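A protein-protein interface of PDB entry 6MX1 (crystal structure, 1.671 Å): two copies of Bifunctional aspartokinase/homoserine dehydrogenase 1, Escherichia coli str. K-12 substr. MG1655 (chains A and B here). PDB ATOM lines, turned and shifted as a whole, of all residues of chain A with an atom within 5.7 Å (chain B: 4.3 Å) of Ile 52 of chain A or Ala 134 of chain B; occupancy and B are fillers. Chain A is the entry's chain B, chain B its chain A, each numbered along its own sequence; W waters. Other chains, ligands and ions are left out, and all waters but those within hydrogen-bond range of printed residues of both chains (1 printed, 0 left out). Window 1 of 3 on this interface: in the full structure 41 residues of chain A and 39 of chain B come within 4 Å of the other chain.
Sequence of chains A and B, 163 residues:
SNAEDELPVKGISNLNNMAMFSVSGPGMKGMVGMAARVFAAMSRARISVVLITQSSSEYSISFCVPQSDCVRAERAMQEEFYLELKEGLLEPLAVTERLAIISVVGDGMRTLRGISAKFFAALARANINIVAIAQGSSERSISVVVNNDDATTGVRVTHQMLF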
ATOM      1  N   PHE A  39     -18.639  19.274  19.158  1.00  0.00           N
ATOM      2  CA  PHE A  39     -17.268  19.567  18.787  1.00  0.00           C
ATOM      3  C   PHE A  39     -17.155  20.417  17.512  1.00  0.00           C
ATOM      4  O   PHE A  39     -16.190  21.204  17.399  1.00  0.00           O
ATOM      5  CB  PHE A  39     -16.504  18.227  18.805  1.00  0.00           C
ATOM      6  CG  PHE A  39     -16.518  17.635  20.186  1.00  0.00           C
ATOM      7  CD1 PHE A  39     -15.982  18.389  21.248  1.00  0.00           C
ATOM      8  CD2 PHE A  39     -17.144  16.449  20.484  1.00  0.00           C
ATOM      9  CE1 PHE A  39     -16.043  17.937  22.577  1.00  0.00           C
ATOM     10  CE2 PHE A  39     -17.218  15.977  21.816  1.00  0.00           C
ATOM     11  CZ  PHE A  39     -16.652  16.720  22.863  1.00  0.00           C
ATOM     12  N   VAL A  49     -10.305  21.717  22.900  1.00  0.00           N
ATOM     13  CA  VAL A  49     -10.930  20.777  23.824  1.00  0.00           C
ATOM     14  C   VAL A  49      -9.834  19.846  24.310  1.00  0.00           C
ATOM     15  O   VAL A  49      -9.232  19.116  23.518  1.00  0.00           O
ATOM     16  CB  VAL A  49     -12.065  20.040  23.125  1.00  0.00           C
ATOM     17  CG1 VAL A  49     -12.567  18.901  23.967  1.00  0.00           C
ATOM     18  CG2 VAL A  49     -13.187  21.051  22.809  1.00  0.00           C
ATOM     19  N   VAL A  50      -9.501  19.905  25.599  1.00  0.00           N
ATOM     20  CA  VAL A  50      -8.314  19.170  26.032  1.00  0.00           C
ATOM     21  C   VAL A  50      -8.658  17.787  26.573  1.00  0.00           C
ATOM     22  O   VAL A  50      -7.760  16.948  26.668  1.00  0.00           O
ATOM     23  CB  VAL A  50      -7.475  19.937  27.071  1.00  0.00           C
ATOM     24  CG1 VAL A  50      -7.303  21.370  26.651  1.00  0.00           C
ATOM     25  CG2 VAL A  50      -8.074  19.808  28.430  1.00  0.00           C
ATOM     26  N   LEU A  51      -9.927  17.520  26.900  1.00  0.00           N
ATOM     27  CA  LEU A  51     -10.320  16.227  27.454  1.00  0.00           C
ATOM     28  C   LEU A  51     -11.756  15.976  27.084  1.00  0.00           C
ATOM     29  O   LEU A  51     -12.571  16.881  27.158  1.00  0.00           O
ATOM     30  CB  LEU A  51     -10.127  16.205  28.986  1.00  0.00           C
ATOM     31  CG  LEU A  51     -10.279  14.840  29.706  1.00  0.00           C
ATOM     32  CD1 LEU A  51      -9.367  14.711  30.882  1.00  0.00           C
ATOM     33  CD2 LEU A  51     -11.740  14.726  30.180  1.00  0.00           C
ATOM     34  N   ILE A  52     -12.064  14.737  26.697  1.00  0.00           N
ATOM     35  CA  ILE A  52     -13.469  14.368  26.409  1.00  0.00           C
ATOM     36  C   ILE A  52     -13.786  13.047  27.101  1.00  0.00           C
ATOM     37  O   ILE A  52     -12.988  12.109  27.041  1.00  0.00           O
ATOM     38  CB  ILE A  52     -13.724  14.208  24.890  1.00  0.00           C
ATOM     39  CG1 ILE A  52     -13.394  15.481  24.106  1.00  0.00           C
ATOM     40  CG2 ILE A  52     -15.208  13.813  24.641  1.00  0.00           C
ATOM     41  CD1 ILE A  52     -13.366  15.225  22.584  1.00  0.00           C
ATOM     42  N   THR A  53     -14.970  12.948  27.724  1.00  0.00           N
ATOM     43  CA  THR A  53     -15.386  11.657  28.265  1.00  0.00           C
ATOM     44  C   THR A  53     -16.888  11.467  28.123  1.00  0.00           C
ATOM     45  O   THR A  53     -17.684  12.367  28.436  1.00  0.00           O
ATOM     46  CB  THR A  53     -14.890  11.437  29.721  1.00  0.00           C
ATOM     47  OG1 THR A  53     -15.584  10.328  30.317  1.00  0.00           O
ATOM     48  CG2 THR A  53     -15.126  12.664  30.640  1.00  0.00           C
ATOM     49  N   GLN A  54     -17.273  10.276  27.656  1.00  0.00           N
ATOM     50  CA  GLN A  54     -18.684   9.870  27.644  1.00  0.00           C
ATOM     51  C   GLN A  54     -18.729   8.436  28.144  1.00  0.00           C
ATOM     52  O   GLN A  54     -18.044   7.545  27.593  1.00  0.00           O
ATOM     53  CB  GLN A  54     -19.284   9.973  26.236  1.00  0.00           C
ATOM     54  CG  GLN A  54     -20.780   9.463  26.152  1.00  0.00           C
ATOM     55  CD  GLN A  54     -21.167   9.063  24.744  1.00  0.00           C
ATOM     56  OE1 GLN A  54     -21.769   7.996  24.524  1.00  0.00           O
ATOM     57  NE2 GLN A  54     -20.917   9.959  23.792  1.00  0.00           N
ATOM     58  N   ILE A  61     -22.074  13.800  27.882  1.00  0.00           N
ATOM     59  CA  ILE A  61     -20.719  14.066  27.376  1.00  0.00           C
ATOM     60  C   ILE A  61     -20.145  15.128  28.264  1.00  0.00           C
ATOM     61  O   ILE A  61     -20.835  16.104  28.551  1.00  0.00           O
ATOM     62  CB  ILE A  61     -20.713  14.545  25.915  1.00  0.00           C
ATOM     63  CG1 ILE A  61     -21.279  13.411  24.993  1.00  0.00           C
ATOM     64  CG2 ILE A  61     -19.246  14.878  25.494  1.00  0.00           C
ATOM     65  CD1 ILE A  61     -21.476  13.930  23.517  1.00  0.00           C
ATOM     66  N   SER A  62     -18.924  14.923  28.758  1.00  0.00           N
ATOM     67  CA  SER A  62     -18.215  15.969  29.495  1.00  0.00           C
ATOM     68  C   SER A  62     -16.955  16.332  28.710  1.00  0.00           C
ATOM     69  O   SER A  62     -16.341  15.457  28.075  1.00  0.00           O
ATOM     70  CB  SER A  62     -17.808  15.526  30.929  1.00  0.00           C
ATOM     71  OG  SER A  62     -18.904  15.393  31.837  1.00  0.00           O
ATOM     72  N   PHE A  63     -16.553  17.614  28.751  1.00  0.00           N
ATOM     73  CA  PHE A  63     -15.296  17.942  28.115  1.00  0.00           C
ATOM     74  C   PHE A  63     -14.716  19.138  28.844  1.00  0.00           C
ATOM     75  O   PHE A  63     -15.454  19.883  29.490  1.00  0.00           O
ATOM     76  CB  PHE A  63     -15.457  18.268  26.607  1.00  0.00           C
ATOM     77  CG  PHE A  63     -16.374  19.459  26.302  1.00  0.00           C
ATOM     78  CD1 PHE A  63     -17.757  19.288  26.178  1.00  0.00           C
ATOM     79  CD2 PHE A  63     -15.838  20.743  26.141  1.00  0.00           C
ATOM     80  CE1 PHE A  63     -18.608  20.386  25.891  1.00  0.00           C
ATOM     81  CE2 PHE A  63     -16.665  21.855  25.858  1.00  0.00           C
ATOM     82  CZ  PHE A  63     -18.069  21.650  25.715  1.00  0.00           C
ATOM     83  N   CYS A  64     -13.403  19.256  28.775  1.00  0.00           N
ATOM     84  CA  CYS A  64     -12.676  20.311  29.492  1.00  0.00           C
ATOM     85  C   CYS A  64     -12.078  21.311  28.526  1.00  0.00           C
ATOM     86  O   CYS A  64     -11.598  20.938  27.444  1.00  0.00           O
ATOM     87  CB  CYS A  64     -11.547  19.710  30.298  1.00  0.00           C
ATOM     88  SG  CYS A  64     -12.105  18.704  31.688  1.00  0.00           S
ATOM     89  N   ILE A 133     -12.606  10.922  34.492  1.00  0.00           N
ATOM     90  CA  ILE A 133     -11.462  10.107  34.116  1.00  0.00           C
ATOM     91  C   ILE A 133     -11.491   9.961  32.611  1.00  0.00           C
ATOM     92  O   ILE A 133     -12.573   9.725  32.037  1.00  0.00           O
ATOM     93  CB  ILE A 133     -11.534   8.725  34.759  1.00  0.00           C
ATOM     94  CG1 ILE A 133     -11.493   8.822  36.268  1.00  0.00           C
ATOM     95  CG2 ILE A 133     -10.371   7.843  34.294  1.00  0.00           C
ATOM     96  CD1 ILE A 133     -11.862   7.480  36.902  1.00  0.00           C
ATOM     97  N   ALA A 134     -10.317  10.043  31.961  1.00  0.00           N
ATOM     98  CA  ALA A 134     -10.251   9.630  30.539  1.00  0.00           C
ATOM     99  C   ALA A 134      -8.932   8.952  30.245  1.00  0.00           C
ATOM    100  O   ALA A 134      -7.847   9.508  30.472  1.00  0.00           O
ATOM    101  CB  ALA A 134     -10.461  10.823  29.581  1.00  0.00           C
ATOM    102  N   GLN A 135      -9.029   7.711  29.719  1.00  0.00           N
ATOM    103  CA  GLN A 135      -7.887   6.939  29.235  1.00  0.00           C
ATOM    104  C   GLN A 135      -8.285   6.339  27.896  1.00  0.00           C
ATOM    105  O   GLN A 135      -9.158   5.452  27.837  1.00  0.00           O
ATOM    106  CB  GLN A 135      -7.443   5.834  30.205  1.00  0.00           C
ATOM    107  CG  GLN A 135      -6.314   4.987  29.623  1.00  0.00           C
ATOM    108  CD  GLN A 135      -6.236   3.562  30.173  1.00  0.00           C
ATOM    109  OE1 GLN A 135      -6.142   3.373  31.372  1.00  0.00           O
ATOM    110  NE2 GLN A 135      -6.287   2.550  29.275  1.00  0.00           N
ATOM    111  N   GLY A 136      -7.685   6.838  26.810  1.00  0.00           N
ATOM    112  CA  GLY A 136      -7.937   6.261  25.506  1.00  0.00           C
ATOM    113  C   GLY A 136      -7.127   4.996  25.317  1.00  0.00           C
ATOM    114  O   GLY A 136      -6.242   4.643  26.133  1.00  0.00           O
ATOM    115  N   LEU B  51      -9.381   0.911  27.986  1.00  0.00           N
ATOM    116  CA  LEU B  51     -10.014   2.222  27.899  1.00  0.00           C
ATOM    117  C   LEU B  51     -10.776   2.437  29.191  1.00  0.00           C
ATOM    118  O   LEU B  51     -11.351   1.486  29.717  1.00  0.00           O
ATOM    119  CB  LEU B  51     -10.961   2.254  26.700  1.00  0.00           C
ATOM    120  CG  LEU B  51     -11.705   3.593  26.544  1.00  0.00           C
ATOM    121  CD1 LEU B  51     -11.875   3.830  25.090  1.00  0.00           C
ATOM    122  CD2 LEU B  51     -13.097   3.636  27.220  1.00  0.00           C
ATOM    123  N   ILE B  52     -10.696   3.662  29.778  1.00  0.00           N
ATOM    124  CA  ILE B  52     -11.445   3.948  31.000  1.00  0.00           C
ATOM    125  C   ILE B  52     -12.059   5.314  30.834  1.00  0.00           C
ATOM    126  O   ILE B  52     -11.402   6.236  30.349  1.00  0.00           O
ATOM    127  CB  ILE B  52     -10.599   4.003  32.296  1.00  0.00           C
ATOM    128  CG1 ILE B  52      -9.734   2.785  32.421  1.00  0.00           C
ATOM    129  CG2 ILE B  52     -11.590   4.135  33.545  1.00  0.00           C
ATOM    130  CD1 ILE B  52      -8.760   2.917  33.557  1.00  0.00           C
ATOM    131  N   THR B  53     -13.310   5.447  31.233  1.00  0.00           N
ATOM    132  CA  THR B  53     -13.931   6.765  31.092  1.00  0.00           C
ATOM    133  C   THR B  53     -14.936   6.963  32.210  1.00  0.00           C
ATOM    134  O   THR B  53     -15.654   6.040  32.611  1.00  0.00           O
ATOM    135  CB  THR B  53     -14.530   6.866  29.647  1.00  0.00           C
ATOM    136  OG1 THR B  53     -15.080   8.167  29.441  1.00  0.00           O
ATOM    137  CG2 THR B  53     -15.608   5.825  29.410  1.00  0.00           C
ATOM    138  N   ILE B 133     -16.739   7.515  24.854  1.00  0.00           N
ATOM    139  CA  ILE B 133     -15.670   8.346  24.291  1.00  0.00           C
ATOM    140  C   ILE B 133     -14.605   8.526  25.352  1.00  0.00           C
ATOM    141  O   ILE B 133     -14.914   8.764  26.515  1.00  0.00           O
ATOM    142  CB  ILE B 133     -16.187   9.749  23.854  1.00  0.00           C
ATOM    143  CG1 ILE B 133     -17.345   9.655  22.806  1.00  0.00           C
ATOM    144  CG2 ILE B 133     -15.011  10.594  23.258  1.00  0.00           C
ATOM    145  CD1 ILE B 133     -17.969  11.047  22.626  1.00  0.00           C
ATOM    146  N   ALA B 134     -13.325   8.466  24.949  1.00  0.00           N
ATOM    147  CA  ALA B 134     -12.296   8.854  25.852  1.00  0.00           C
ATOM    148  C   ALA B 134     -11.228   9.606  25.075  1.00  0.00           C
ATOM    149  O   ALA B 134     -10.654   9.055  24.133  1.00  0.00           O
ATOM    150  CB  ALA B 134     -11.668   7.646  26.578  1.00  0.00           C
ATOM    151  N   GLN B 135     -10.928  10.828  25.496  1.00  0.00           N
ATOM    152  CA  GLN B 135      -9.746  11.548  25.022  1.00  0.00           C
ATOM    153  C   GLN B 135      -9.074  12.141  26.242  1.00  0.00           C
ATOM    154  O   GLN B 135      -9.645  13.000  26.904  1.00  0.00           O
ATOM    155  CB  GLN B 135     -10.109  12.684  24.039  1.00  0.00           C
ATOM    156  CG  GLN B 135      -8.905  13.477  23.623  1.00  0.00           C
ATOM    157  CD  GLN B 135      -9.251  14.902  23.248  1.00  0.00           C
ATOM    158  OE1 GLN B 135      -9.970  15.113  22.315  1.00  0.00           O
ATOM    159  NE2 GLN B 135      -8.719  15.882  23.988  1.00  0.00           N
ATOM    160  N   GLY B 136      -7.805  11.713  26.530  1.00  0.00           N
ATOM    161  CA  GLY B 136      -7.032  12.316  27.585  1.00  0.00           C
ATOM    162  C   GLY B 136      -6.367  13.602  27.144  1.00  0.00           C
ATOM    163  O   GLY B 136      -6.429  13.984  25.976  1.00  0.00           O
ATOM    164  N   ILE B 142      -8.043  10.372  20.233  1.00  0.00           N
ATOM    165  CA  ILE B 142      -9.428  10.269  20.664  1.00  0.00           C
ATOM    166  C   ILE B 142      -9.877   8.853  20.356  1.00  0.00           C
ATOM    167  O   ILE B 142      -9.669   8.371  19.225  1.00  0.00           O
ATOM    168  CB  ILE B 142     -10.356  11.243  19.929  1.00  0.00           C
ATOM    169  CG1 ILE B 142      -9.902  12.684  20.046  1.00  0.00           C
ATOM    170  CG2 ILE B 142     -11.823  11.067  20.366  1.00  0.00           C
ATOM    171  CD1 ILE B 142     -10.563  13.542  18.967  1.00  0.00           C
ATOM    172  N   SER B 143     -10.476   8.181  21.345  1.00  0.00           N
ATOM    173  CA  SER B 143     -11.005   6.822  21.162  1.00  0.00           C
ATOM    174  C   SER B 143     -12.506   6.821  21.334  1.00  0.00           C
ATOM    175  O   SER B 143     -13.048   7.481  22.222  1.00  0.00           O
ATOM    176  CB  SER B 143     -10.387   5.825  22.158  1.00  0.00           C
ATOM    177  OG  SER B 143      -9.000   5.709  22.047  1.00  0.00           O
HETATM  178  O   HOH W   1     -10.586  17.352  21.041  1.00  0.00           O
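Among the printed residues, merely in contact across the chains: Gln 135 of chain A with Leu 51 of chain B, Leu 51 of chain A with Gln 135 of chain B, Ile 133 of chain A with Thr 53 of chain B, Thr 53 of chain A with Ile 133 of chain B, Gln 54 of chain A with Thr 53 of chain B, Ile 52 of chain A with Ile 133 of chain B, Ile 52 of chain A with Ala 134 of chain B, Ala 134 of chain A with Gln 135 of chain B, Gln 135 of chain A with Ala 134 of chain B, Ala 134 of chain A with Ile 52 of chain B, Gly 136 of chain A with Ser 143 of chain B and Ile 133 of chain A with Ile 52 of chain B.
Water W1 lies within hydrogen-bond range of the side-chain amide oxygen (OE1) of Gln 135 of chain B (2.6 Å) and the backbone carbonyl oxygen (O) of Val 49 of chain A (3.3 Å).
Printed residues of chain B within 4 Å of Val 49 of chain A: Gln 135.
Ile 52 of chain A touches just these residues of chain B: Ile 133 (3.5 Å), Ala 134 (3.5 Å) and Gln 135 (2.9 Å).
Of the printed residues of chain B, Gly 136 of chain A touches Ser 143.
Ala 134 of chain B touches two residues of chain A.
The nearest printed residue of chain B that does not touch Ile 52 of chain A is Ile 142 of chain B (4.9 Å).
The nearest residue of chain A that does not touch Ala 134 of chain B is Gly 136 of chain A (4.1 Å).
The nearest printed residue of chain A that does not touch Ile 52 of chain B is Gly 136 of chain A (5.2 Å).
The side-chain hydroxyl (OG1) of Thr 53 of chain B sits at hydrogen-bond distance from the backbone carbonyl oxygen (O) of Ile 133 of chain B, at 3.0 Å.
The backbone NH (N) of Ala 134 of chain B sits at hydrogen-bond distance from the backbone carbonyl oxygen (O) of Ser 143 of chain B.
O of Cys 64 of chain A is in hydrogen-bond range of N of Val 50 of chain A.
The backbone NH of Cys 64 of chain A lies within hydrogen-bond range of the backbone carbonyl oxygen of Leu 51 of chain A.
The backbone NH (N) of Ser 62 of chain A is in hydrogen-bond range of the backbone carbonyl oxygen (O) of Thr 53 of chain A (2.9 Å).
Printed residues of chain A that touch a printed residue of chain B: Val 49, Val 50, Leu 51, Ile 52, Thr 53, Gln 54, Ile 133, Ala 134, Gln 135 and Gly 136.
Hydrophobic or aromatic side chains of chain A that line the printed part of chain B: Leu 51, Ile 52, Ile 133 and Ala 134.
Printed residues of chain B that touch a printed residue of chain A: Leu 51, Ile 52, Thr 53, Ile 133, Ala 134, Gln 135, Gly 136 and Ser 143.
Among the printed residues, 19 pairs touch across the chains.
Ile 52 of chain A touches Ile 133 of chain B, and with the chains exchanged Ile 133 of chain A touches Ile 52 of chain B.
Thr 53 of chain B touches its own counterpart, Thr 53 of chain A.
Thr 53 of chain A touches Ile 133 of chain B, and with the chains exchanged Ile 133 of chain A touches Thr 53 of chain B.
Ala 134 of chain A touches Gln 135 of chain B, and with the chains exchanged Gln 135 of chain A touches Ala 134 of chain B.
7 positions are printed for both chains.
Of the 19 pairs that touch across the chains among the printed residues, 13 have their exchanged pair printed and touching as well.
The backbone carbonyl oxygen (O) of Ile 52 of chain B sits at hydrogen-bond distance from the backbone NH (N) of Gln 135 of chain A, at 2.9 Å.
N of Gln 54 of chain A is in hydrogen-bond range of O of Ile 133 of chain B, 3.0 Å away.
The backbone carbonyl oxygen (O) of Val 49 of chain A lies within hydrogen-bond range of the side-chain amide nitrogen (NE2) of Gln 135 of chain B.
O of Val 50 of chain A is in hydrogen-bond range of NE2 of Gln 135 of chain B.
N of Gln 135 of chain B sits at hydrogen-bond distance from O of Ile 52 of chain A (2.9 Å).
The backbone carbonyl oxygen (O) of Val 50 of chain A sits close to the backbone carbonyl oxygen (O) of Gly 136 of chain B, 3.3 Å away.
OG1 of Thr 53 of chain B sits close to OG1 of Thr 53 of chain A (2.4 Å).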
